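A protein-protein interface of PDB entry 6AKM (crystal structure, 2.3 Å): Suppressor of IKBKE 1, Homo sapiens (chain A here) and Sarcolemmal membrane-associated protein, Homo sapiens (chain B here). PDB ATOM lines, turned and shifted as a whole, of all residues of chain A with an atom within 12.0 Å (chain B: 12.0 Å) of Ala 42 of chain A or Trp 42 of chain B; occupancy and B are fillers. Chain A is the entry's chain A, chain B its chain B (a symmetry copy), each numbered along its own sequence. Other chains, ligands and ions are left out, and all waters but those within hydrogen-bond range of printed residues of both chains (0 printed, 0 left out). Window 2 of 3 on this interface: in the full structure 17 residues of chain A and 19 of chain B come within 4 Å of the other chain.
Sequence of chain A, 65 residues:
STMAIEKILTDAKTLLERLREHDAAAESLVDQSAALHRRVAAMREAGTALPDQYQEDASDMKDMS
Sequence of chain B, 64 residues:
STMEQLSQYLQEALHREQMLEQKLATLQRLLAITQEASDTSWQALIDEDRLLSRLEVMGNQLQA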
ATOM      1  N   SER A  33      -4.871 -37.850 -16.908  1.00  0.00           N
ATOM      2  CA  SER A  33      -5.609 -38.175 -18.125  1.00  0.00           C
ATOM      3  C   SER A  33      -6.820 -37.278 -18.294  1.00  0.00           C
ATOM      4  O   SER A  33      -7.205 -36.991 -19.425  1.00  0.00           O
ATOM      5  CB  SER A  33      -6.049 -39.632 -18.111  1.00  0.00           C
ATOM      6  OG  SER A  33      -7.064 -39.754 -17.155  1.00  0.00           O
ATOM      7  N   ALA A  34      -7.417 -36.818 -17.187  1.00  0.00           N
ATOM      8  CA  ALA A  34      -8.509 -35.853 -17.267  1.00  0.00           C
ATOM      9  C   ALA A  34      -8.040 -34.542 -17.882  1.00  0.00           C
ATOM     10  O   ALA A  34      -8.749 -33.958 -18.712  1.00  0.00           O
ATOM     11  CB  ALA A  34      -9.108 -35.600 -15.883  1.00  0.00           C
ATOM     12  N   ALA A  35      -6.845 -34.071 -17.497  1.00  0.00           N
ATOM     13  CA  ALA A  35      -6.296 -32.848 -18.095  1.00  0.00           C
ATOM     14  C   ALA A  35      -6.048 -33.045 -19.579  1.00  0.00           C
ATOM     15  O   ALA A  35      -6.292 -32.146 -20.393  1.00  0.00           O
ATOM     16  CB  ALA A  35      -4.993 -32.441 -17.399  1.00  0.00           C
ATOM     17  N   LEU A  36      -5.565 -34.224 -19.948  1.00  0.00           N
ATOM     18  CA  LEU A  36      -5.388 -34.537 -21.357  1.00  0.00           C
ATOM     19  C   LEU A  36      -6.729 -34.577 -22.073  1.00  0.00           C
ATOM     20  O   LEU A  36      -6.866 -34.040 -23.178  1.00  0.00           O
ATOM     21  CB  LEU A  36      -4.663 -35.874 -21.496  1.00  0.00           C
ATOM     22  CG  LEU A  36      -4.322 -36.356 -22.901  1.00  0.00           C
ATOM     23  CD1 LEU A  36      -3.483 -35.284 -23.655  1.00  0.00           C
ATOM     24  CD2 LEU A  36      -3.608 -37.701 -22.794  1.00  0.00           C
ATOM     25  N   HIS A  37      -7.733 -35.201 -21.451  1.00  0.00           N
ATOM     26  CA  HIS A  37      -9.065 -35.201 -22.035  1.00  0.00           C
ATOM     27  C   HIS A  37      -9.523 -33.773 -22.304  1.00  0.00           C
ATOM     28  O   HIS A  37      -9.977 -33.448 -23.406  1.00  0.00           O
ATOM     29  CB  HIS A  37     -10.069 -35.895 -21.117  1.00  0.00           C
ATOM     30  CG  HIS A  37     -11.481 -35.721 -21.571  1.00  0.00           C
ATOM     31  ND1 HIS A  37     -12.376 -34.904 -20.921  1.00  0.00           N
ATOM     32  CD2 HIS A  37     -12.134 -36.211 -22.651  1.00  0.00           C
ATOM     33  CE1 HIS A  37     -13.527 -34.905 -21.573  1.00  0.00           C
ATOM     34  NE2 HIS A  37     -13.406 -35.692 -22.626  1.00  0.00           N
ATOM     35  N   ARG A  38      -9.412 -32.904 -21.291  1.00  0.00           N
ATOM     36  CA  ARG A  38      -9.823 -31.515 -21.465  1.00  0.00           C
ATOM     37  C   ARG A  38      -9.090 -30.875 -22.633  1.00  0.00           C
ATOM     38  O   ARG A  38      -9.684 -30.128 -23.420  1.00  0.00           O
ATOM     39  CB  ARG A  38      -9.574 -30.716 -20.183  1.00  0.00           C
ATOM     40  CG  ARG A  38     -10.182 -29.329 -20.227  1.00  0.00           C
ATOM     41  CD  ARG A  38      -9.517 -28.408 -19.233  1.00  0.00           C
ATOM     42  NE  ARG A  38      -9.997 -28.658 -17.878  1.00  0.00           N
ATOM     43  CZ  ARG A  38     -11.221 -28.366 -17.442  1.00  0.00           C
ATOM     44  NH1 ARG A  38     -12.108 -27.790 -18.250  1.00  0.00           N
ATOM     45  NH2 ARG A  38     -11.557 -28.642 -16.188  1.00  0.00           N
ATOM     46  N   ARG A  39      -7.796 -31.159 -22.769  1.00  0.00           N
ATOM     47  CA  ARG A  39      -7.056 -30.495 -23.828  1.00  0.00           C
ATOM     48  C   ARG A  39      -7.494 -31.006 -25.199  1.00  0.00           C
ATOM     49  O   ARG A  39      -7.669 -30.213 -26.126  1.00  0.00           O
ATOM     50  CB  ARG A  39      -5.554 -30.661 -23.609  1.00  0.00           C
ATOM     51  CG  ARG A  39      -4.714 -30.514 -24.875  1.00  0.00           C
ATOM     52  CD  ARG A  39      -4.603 -29.034 -25.246  1.00  0.00           C
ATOM     53  NE  ARG A  39      -3.988 -28.188 -24.225  1.00  0.00           N
ATOM     54  CZ  ARG A  39      -2.687 -28.133 -23.951  1.00  0.00           C
ATOM     55  NH1 ARG A  39      -1.812 -28.840 -24.655  1.00  0.00           N
ATOM     56  NH2 ARG A  39      -2.259 -27.322 -22.994  1.00  0.00           N
ATOM     57  N   VAL A  40      -7.728 -32.315 -25.336  1.00  0.00           N
ATOM     58  CA  VAL A  40      -8.156 -32.853 -26.628  1.00  0.00           C
ATOM     59  C   VAL A  40      -9.554 -32.348 -26.983  1.00  0.00           C
ATOM     60  O   VAL A  40      -9.825 -31.995 -28.136  1.00  0.00           O
ATOM     61  CB  VAL A  40      -8.079 -34.392 -26.621  1.00  0.00           C
ATOM     62  CG1 VAL A  40      -8.745 -34.997 -27.884  1.00  0.00           C
ATOM     63  CG2 VAL A  40      -6.629 -34.836 -26.534  1.00  0.00           C
ATOM     64  N   ALA A  41     -10.449 -32.263 -25.996  1.00  0.00           N
ATOM     65  CA  ALA A  41     -11.797 -31.779 -26.269  1.00  0.00           C
ATOM     66  C   ALA A  41     -11.786 -30.304 -26.653  1.00  0.00           C
ATOM     67  O   ALA A  41     -12.560 -29.873 -27.519  1.00  0.00           O
ATOM     68  CB  ALA A  41     -12.693 -32.008 -25.050  1.00  0.00           C
ATOM     69  N   ALA A  42     -10.916 -29.518 -26.023  1.00  0.00           N
ATOM     70  CA  ALA A  42     -10.820 -28.103 -26.364  1.00  0.00           C
ATOM     71  C   ALA A  42     -10.218 -27.896 -27.753  1.00  0.00           C
ATOM     72  O   ALA A  42     -10.605 -26.954 -28.455  1.00  0.00           O
ATOM     73  CB  ALA A  42     -10.016 -27.354 -25.301  1.00  0.00           C
ATOM     74  N   MET A  43      -9.277 -28.753 -28.171  1.00  0.00           N
ATOM     75  CA  MET A  43      -8.808 -28.690 -29.554  1.00  0.00           C
ATOM     76  C   MET A  43      -9.949 -28.995 -30.516  1.00  0.00           C
ATOM     77  O   MET A  43     -10.092 -28.338 -31.552  1.00  0.00           O
ATOM     78  CB  MET A  43      -7.641 -29.660 -29.783  1.00  0.00           C
ATOM     79  CG  MET A  43      -6.256 -29.163 -29.311  1.00  0.00           C
ATOM     80  SD  MET A  43      -5.019 -30.487 -29.018  1.00  0.00           S
ATOM     81  CE  MET A  43      -4.700 -31.052 -30.688  1.00  0.00           C
ATOM     82  N   ARG A  44     -10.802 -29.925 -30.189  1.00  0.00           N
ATOM     83  CA  ARG A  44     -11.901 -30.246 -31.121  1.00  0.00           C
ATOM     84  C   ARG A  44     -12.907 -29.102 -31.153  1.00  0.00           C
ATOM     85  O   ARG A  44     -13.021 -28.480 -32.185  1.00  0.00           O
ATOM     86  CB  ARG A  44     -12.610 -31.522 -30.689  1.00  0.00           C
ATOM     87  CG  ARG A  44     -13.895 -31.747 -31.453  1.00  0.00           C
ATOM     88  CD  ARG A  44     -14.531 -33.013 -30.977  1.00  0.00           C
ATOM     89  NE  ARG A  44     -15.137 -32.735 -29.699  1.00  0.00           N
ATOM     90  CZ  ARG A  44     -15.222 -33.625 -28.744  1.00  0.00           C
ATOM     91  NH1 ARG A  44     -15.919 -34.729 -28.927  1.00  0.00           N
ATOM     92  NH2 ARG A  44     -14.557 -33.427 -27.633  1.00  0.00           N
ATOM     93  N   GLU A  45     -13.308 -28.622 -30.010  1.00  0.00           N
ATOM     94  CA  GLU A  45     -14.267 -27.522 -30.036  1.00  0.00           C
ATOM     95  C   GLU A  45     -13.686 -26.283 -30.710  1.00  0.00           C
ATOM     96  O   GLU A  45     -14.417 -25.550 -31.392  1.00  0.00           O
ATOM     97  CB  GLU A  45     -14.738 -27.197 -28.615  1.00  0.00           C
ATOM     98  N   ALA A  46     -12.382 -26.031 -30.549  1.00  0.00           N
ATOM     99  CA  ALA A  46     -11.757 -24.907 -31.244  1.00  0.00           C
ATOM    100  C   ALA A  46     -11.582 -25.167 -32.734  1.00  0.00           C
ATOM    101  O   ALA A  46     -11.250 -24.233 -33.474  1.00  0.00           O
ATOM    102  CB  ALA A  46     -10.401 -24.567 -30.621  1.00  0.00           C
ATOM    103  N   GLY A  47     -11.790 -26.400 -33.188  1.00  0.00           N
ATOM    104  CA  GLY A  47     -11.857 -26.719 -34.598  1.00  0.00           C
ATOM    105  C   GLY A  47     -13.258 -26.842 -35.159  1.00  0.00           C
ATOM    106  O   GLY A  47     -13.406 -27.188 -36.337  1.00  0.00           O
ATOM    107  N   THR A  48     -14.289 -26.574 -34.361  1.00  0.00           N
ATOM    108  CA  THR A  48     -15.682 -26.710 -34.786  1.00  0.00           C
ATOM    109  C   THR A  48     -16.269 -25.346 -35.140  1.00  0.00           C
ATOM    110  O   THR A  48     -16.807 -25.159 -36.230  1.00  0.00           O
ATOM    111  CB  THR A  48     -16.552 -27.378 -33.685  1.00  0.00           C
ATOM    112  OG1 THR A  48     -16.354 -28.800 -33.697  1.00  0.00           O
ATOM    113  CG2 THR A  48     -18.029 -27.072 -33.898  1.00  0.00           C
ATOM    114  N   ILE B  33       4.164 -37.097 -22.115  1.00  0.00           N
ATOM    115  CA  ILE B  33       4.647 -36.729 -23.442  1.00  0.00           C
ATOM    116  C   ILE B  33       3.496 -36.588 -24.432  1.00  0.00           C
ATOM    117  O   ILE B  33       3.604 -35.834 -25.409  1.00  0.00           O
ATOM    118  CB  ILE B  33       5.742 -37.706 -23.922  1.00  0.00           C
ATOM    119  CG1 ILE B  33       5.188 -39.072 -24.277  1.00  0.00           C
ATOM    120  CG2 ILE B  33       6.877 -37.781 -22.905  1.00  0.00           C
ATOM    121  CD1 ILE B  33       6.199 -39.934 -25.057  1.00  0.00           C
ATOM    122  N   THR B  34       2.362 -37.245 -24.185  1.00  0.00           N
ATOM    123  CA  THR B  34       1.178 -36.944 -24.986  1.00  0.00           C
ATOM    124  C   THR B  34       0.648 -35.540 -24.688  1.00  0.00           C
ATOM    125  O   THR B  34       0.222 -34.818 -25.601  1.00  0.00           O
ATOM    126  CB  THR B  34       0.108 -38.006 -24.746  1.00  0.00           C
ATOM    127  OG1 THR B  34       0.713 -39.303 -24.855  1.00  0.00           O
ATOM    128  CG2 THR B  34      -1.026 -37.883 -25.750  1.00  0.00           C
ATOM    129  N   GLN B  35       0.677 -35.128 -23.425  1.00  0.00           N
ATOM    130  CA  GLN B  35       0.220 -33.787 -23.095  1.00  0.00           C
ATOM    131  C   GLN B  35       1.078 -32.733 -23.787  1.00  0.00           C
ATOM    132  O   GLN B  35       0.554 -31.781 -24.375  1.00  0.00           O
ATOM    133  CB  GLN B  35       0.216 -33.592 -21.578  1.00  0.00           C
ATOM    134  CG  GLN B  35      -0.194 -32.197 -21.133  1.00  0.00           C
ATOM    135  CD  GLN B  35      -1.667 -31.916 -21.337  1.00  0.00           C
ATOM    136  OE1 GLN B  35      -2.509 -32.771 -21.074  1.00  0.00           O
ATOM    137  NE2 GLN B  35      -1.986 -30.715 -21.825  1.00  0.00           N
ATOM    138  N   GLU B  36       2.364 -32.908 -23.769  1.00  0.00           N
ATOM    139  CA  GLU B  36       3.255 -31.946 -24.414  1.00  0.00           C
ATOM    140  C   GLU B  36       3.209 -32.111 -25.923  1.00  0.00           C
ATOM    141  O   GLU B  36       3.345 -31.166 -26.574  1.00  0.00           O
ATOM    142  CB  GLU B  36       4.591 -31.815 -23.711  1.00  0.00           C
ATOM    143  CG  GLU B  36       5.547 -32.941 -23.877  1.00  0.00           C
ATOM    144  CD  GLU B  36       6.482 -33.083 -22.683  1.00  0.00           C
ATOM    145  OE1 GLU B  36       6.625 -32.121 -21.937  1.00  0.00           O
ATOM    146  OE2 GLU B  36       7.059 -34.151 -22.490  1.00  0.00           O
ATOM    147  N   ALA B  37       2.913 -33.245 -26.430  1.00  0.00           N
ATOM    148  CA  ALA B  37       2.821 -33.391 -27.877  1.00  0.00           C
ATOM    149  C   ALA B  37       1.656 -32.590 -28.449  1.00  0.00           C
ATOM    150  O   ALA B  37       1.673 -32.234 -29.631  1.00  0.00           O
ATOM    151  CB  ALA B  37       2.680 -34.865 -28.263  1.00  0.00           C
ATOM    152  N   SER B  38       0.633 -32.315 -27.640  1.00  0.00           N
ATOM    153  CA  SER B  38      -0.527 -31.578 -28.119  1.00  0.00           C
ATOM    154  C   SER B  38      -0.314 -30.072 -28.097  1.00  0.00           C
ATOM    155  O   SER B  38      -1.112 -29.341 -28.695  1.00  0.00           O
ATOM    156  CB  SER B  38      -1.747 -31.931 -27.277  1.00  0.00           C
ATOM    157  OG  SER B  38      -1.631 -31.346 -25.996  1.00  0.00           O
ATOM    158  N   ASP B  39       0.760 -29.607 -27.451  1.00  0.00           N
ATOM    159  CA  ASP B  39       0.890 -28.188 -27.151  1.00  0.00           C
ATOM    160  C   ASP B  39       0.976 -27.352 -28.417  1.00  0.00           C
ATOM    161  O   ASP B  39       0.365 -26.282 -28.495  1.00  0.00           O
ATOM    162  CB  ASP B  39       2.106 -27.949 -26.259  1.00  0.00           C
ATOM    163  CG  ASP B  39       1.817 -28.239 -24.791  1.00  0.00           C
ATOM    164  OD1 ASP B  39       0.638 -28.498 -24.445  1.00  0.00           O
ATOM    165  OD2 ASP B  39       2.770 -28.189 -23.982  1.00  0.00           O
ATOM    166  N   THR B  40       1.703 -27.834 -29.389  1.00  0.00           N
ATOM    167  CA  THR B  40       1.936 -27.109 -30.654  1.00  0.00           C
ATOM    168  C   THR B  40       0.638 -26.993 -31.439  1.00  0.00           C
ATOM    169  O   THR B  40       0.395 -25.946 -31.972  1.00  0.00           O
ATOM    170  CB  THR B  40       3.040 -27.794 -31.453  1.00  0.00           C
ATOM    171  OG1 THR B  40       3.989 -26.791 -31.738  1.00  0.00           O
ATOM    172  CG2 THR B  40       2.586 -28.336 -32.770  1.00  0.00           C
ATOM    173  N   SER B  41      -0.103 -28.055 -31.534  1.00  0.00           N
ATOM    174  CA  SER B  41      -1.384 -28.017 -32.231  1.00  0.00           C
ATOM    175  C   SER B  41      -2.353 -27.091 -31.510  1.00  0.00           C
ATOM    176  O   SER B  41      -3.028 -26.268 -32.142  1.00  0.00           O
ATOM    177  CB  SER B  41      -1.973 -29.425 -32.341  1.00  0.00           C
ATOM    178  OG  SER B  41      -0.997 -30.365 -32.741  1.00  0.00           O
ATOM    179  N   TRP B  42      -2.407 -27.204 -30.179  1.00  0.00           N
ATOM    180  CA  TRP B  42      -3.287 -26.358 -29.381  1.00  0.00           C
ATOM    181  C   TRP B  42      -2.925 -24.884 -29.538  1.00  0.00           C
ATOM    182  O   TRP B  42      -3.813 -24.030 -29.668  1.00  0.00           O
ATOM    183  CB  TRP B  42      -3.230 -26.798 -27.913  1.00  0.00           C
ATOM    184  CG  TRP B  42      -3.930 -25.873 -26.960  1.00  0.00           C
ATOM    185  CD1 TRP B  42      -3.382 -25.247 -25.875  1.00  0.00           C
ATOM    186  CD2 TRP B  42      -5.309 -25.463 -27.005  1.00  0.00           C
ATOM    187  NE1 TRP B  42      -4.332 -24.471 -25.245  1.00  0.00           N
ATOM    188  CE2 TRP B  42      -5.520 -24.587 -25.918  1.00  0.00           C
ATOM    189  CE3 TRP B  42      -6.380 -25.748 -27.861  1.00  0.00           C
ATOM    190  CZ2 TRP B  42      -6.762 -23.997 -25.663  1.00  0.00           C
ATOM    191  CZ3 TRP B  42      -7.613 -25.158 -27.605  1.00  0.00           C
ATOM    192  CH2 TRP B  42      -7.792 -24.295 -26.515  1.00  0.00           C
ATOM    193  N   GLN B  43      -1.623 -24.569 -29.550  1.00  0.00           N
ATOM    194  CA  GLN B  43      -1.189 -23.189 -29.764  1.00  0.00           C
ATOM    195  C   GLN B  43      -1.605 -22.688 -31.143  1.00  0.00           C
ATOM    196  O   GLN B  43      -1.990 -21.526 -31.300  1.00  0.00           O
ATOM    197  CB  GLN B  43       0.329 -23.075 -29.597  1.00  0.00           C
ATOM    198  CG  GLN B  43       0.854 -23.250 -28.169  1.00  0.00           C
ATOM    199  CD  GLN B  43       0.457 -22.117 -27.241  1.00  0.00           C
ATOM    200  OE1 GLN B  43      -0.194 -22.341 -26.217  1.00  0.00           O
ATOM    201  NE2 GLN B  43       0.850 -20.891 -27.591  1.00  0.00           N
ATOM    202  N   ALA B  44      -1.550 -23.559 -32.155  1.00  0.00           N
ATOM    203  CA  ALA B  44      -1.928 -23.166 -33.509  1.00  0.00           C
ATOM    204  C   ALA B  44      -3.393 -22.751 -33.610  1.00  0.00           C
ATOM    205  O   ALA B  44      -3.760 -22.031 -34.544  1.00  0.00           O
ATOM    206  CB  ALA B  44      -1.633 -24.312 -34.481  1.00  0.00           C
ATOM    207  N   LEU B  45      -4.238 -23.189 -32.680  1.00  0.00           N
ATOM    208  CA  LEU B  45      -5.633 -22.770 -32.642  1.00  0.00           C
ATOM    209  C   LEU B  45      -5.866 -21.592 -31.706  1.00  0.00           C
ATOM    210  O   LEU B  45      -6.987 -21.075 -31.659  1.00  0.00           O
ATOM    211  CB  LEU B  45      -6.525 -23.949 -32.222  1.00  0.00           C
ATOM    212  N   ILE B  46      -4.834 -21.161 -30.980  1.00  0.00           N
ATOM    213  CA  ILE B  46      -4.912 -20.101 -29.972  1.00  0.00           C
ATOM    214  C   ILE B  46      -5.940 -20.445 -28.903  1.00  0.00           C
ATOM    215  O   ILE B  46      -5.581 -20.713 -27.758  1.00  0.00           O
ATOM    216  CB  ILE B  46      -5.214 -18.725 -30.608  1.00  0.00           C
ATOM    217  CG1 ILE B  46      -3.980 -18.204 -31.350  1.00  0.00           C
ATOM    218  CG2 ILE B  46      -5.664 -17.737 -29.537  1.00  0.00           C
ATOM    219  CD1 ILE B  46      -3.951 -16.685 -31.519  1.00  0.00           C
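The side-chain amide nitrogen (NE2) of Gln 35 of chain B sits close to the guanidinium group (NH1) of Arg 39 of chain A (3.4 Å).
The guanidinium group (NH1) of Arg 39 of chain A sits at hydrogen-bond distance from the side-chain hydroxyl (OG) of Ser 38 of chain B (2.8 Å).
The guanidinium group (NH1) of Arg 39 of chain A lies within salt-bridge range of the side-chain carboxylate (OD1) of Asp 39 of chain B.
Ala 35 of chain A touches Gln 35 of chain B (C to OE1, 3.9 Å).
Leu 36 of chain A touches Thr 34 of chain B (CD2 to CG2, 3.9 Å).
Gln 35 of chain B touches Leu 36 of chain A.
CD1 of Trp 42 of chain B touches NE of Arg 39 of chain A, 3.4 Å away.
O of Ala 42 of chain A touches CZ3 of Trp 42 of chain B (3.6 Å).
SD of Met 43 of chain A touches CB of Ser 38 of chain B (3.98 Å).
Met 43 of chain A touches Ser 41 of chain B (CE to CB, 3.6 Å).
Met 43 of chain A touches Trp 42 of chain B.
Of the 16 printed residues of chain A, 5 touch a printed residue of chain B.
Along chain A the printed residues that touch a printed residue of chain B span positions 35 to 43.
Printed residues of chain B that touch a printed residue of chain A: Thr 34, Gln 35, Ser 38, Asp 39, Ser 41 and Trp 42.
Hydrophobic or aromatic side chains of chain B that line the printed part of chain A: Trp 42.
Along chain B the printed residues that touch a printed residue of chain A span positions 34 to 42.
Among the printed residues, 11 pairs touch across the chains.
Among the printed residues, Asp or Glu carboxylates within 4 Å of a Lys or Arg side-chain nitrogen of the other chain: Arg 39 of chain A with Asp 39 of chain B.
The backbone carbonyl oxygen (O) of Gln 35 of chain B sits at hydrogen-bond distance from the side-chain hydroxyl (OG) of Ser 38 of chain B (2.8 Å).
Ala 34 of chain A touches none of the printed residues of chain B.
Printed residues of chain B within 4 Å of Ala 35 of chain A: Gln 35 (3.9 Å).
Printed residues of chain B within 4 Å of Leu 36 of chain A: Thr 34 (3.9 Å) and Gln 35 (3.4 Å).
Of chain B, only Gln 35, Ser 38, Asp 39 and Trp 42 come within 4 Å of Arg 39 of chain A.
No residue of chain B comes within 4 Å of Val 40 of chain A.
Ala 42 of chain A touches just one residue of chain B: Trp 42 (3.6 Å).
Met 43 of chain A touches just these residues of chain B: Ser 38, Ser 41 and Trp 42.
No residue of chain B comes within 4 Å of Glu 45 of chain A.
No residue of chain B comes within 4 Å of Ala 46 of chain A.
Printed residues of chain A within 4 Å of Thr 34 of chain B: Leu 36 (3.9 Å).
Of chain A, only Arg 39 (2.5 Å) comes within 4 Å of Asp 39 of chain B.
No residue of chain A comes within 4 Å of Thr 40 of chain B.
Ser 41 of chain B touches just one residue of chain A: Met 43.
Trp 42 of chain B touches just these residues of chain A: Arg 39, Ala 42 and Met 43.
No residue of chain A comes within 4 Å of Gln 43 of chain B.
Leu 45 of chain B touches none of the printed residues of chain A.
No residue of chain A comes within 4 Å of Ile 46 of chain B.
The nearest residue of chain B that does not touch Ala 42 of chain A is Leu 45 of chain B (6.3 Å).
The nearest residue of chain A that does not touch Trp 42 of chain B is Ala 46 of chain A (4.1 Å).
The nearest printed residue of chain B that does not touch Leu 36 of chain A is Ser 38 of chain B (4.9 Å).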
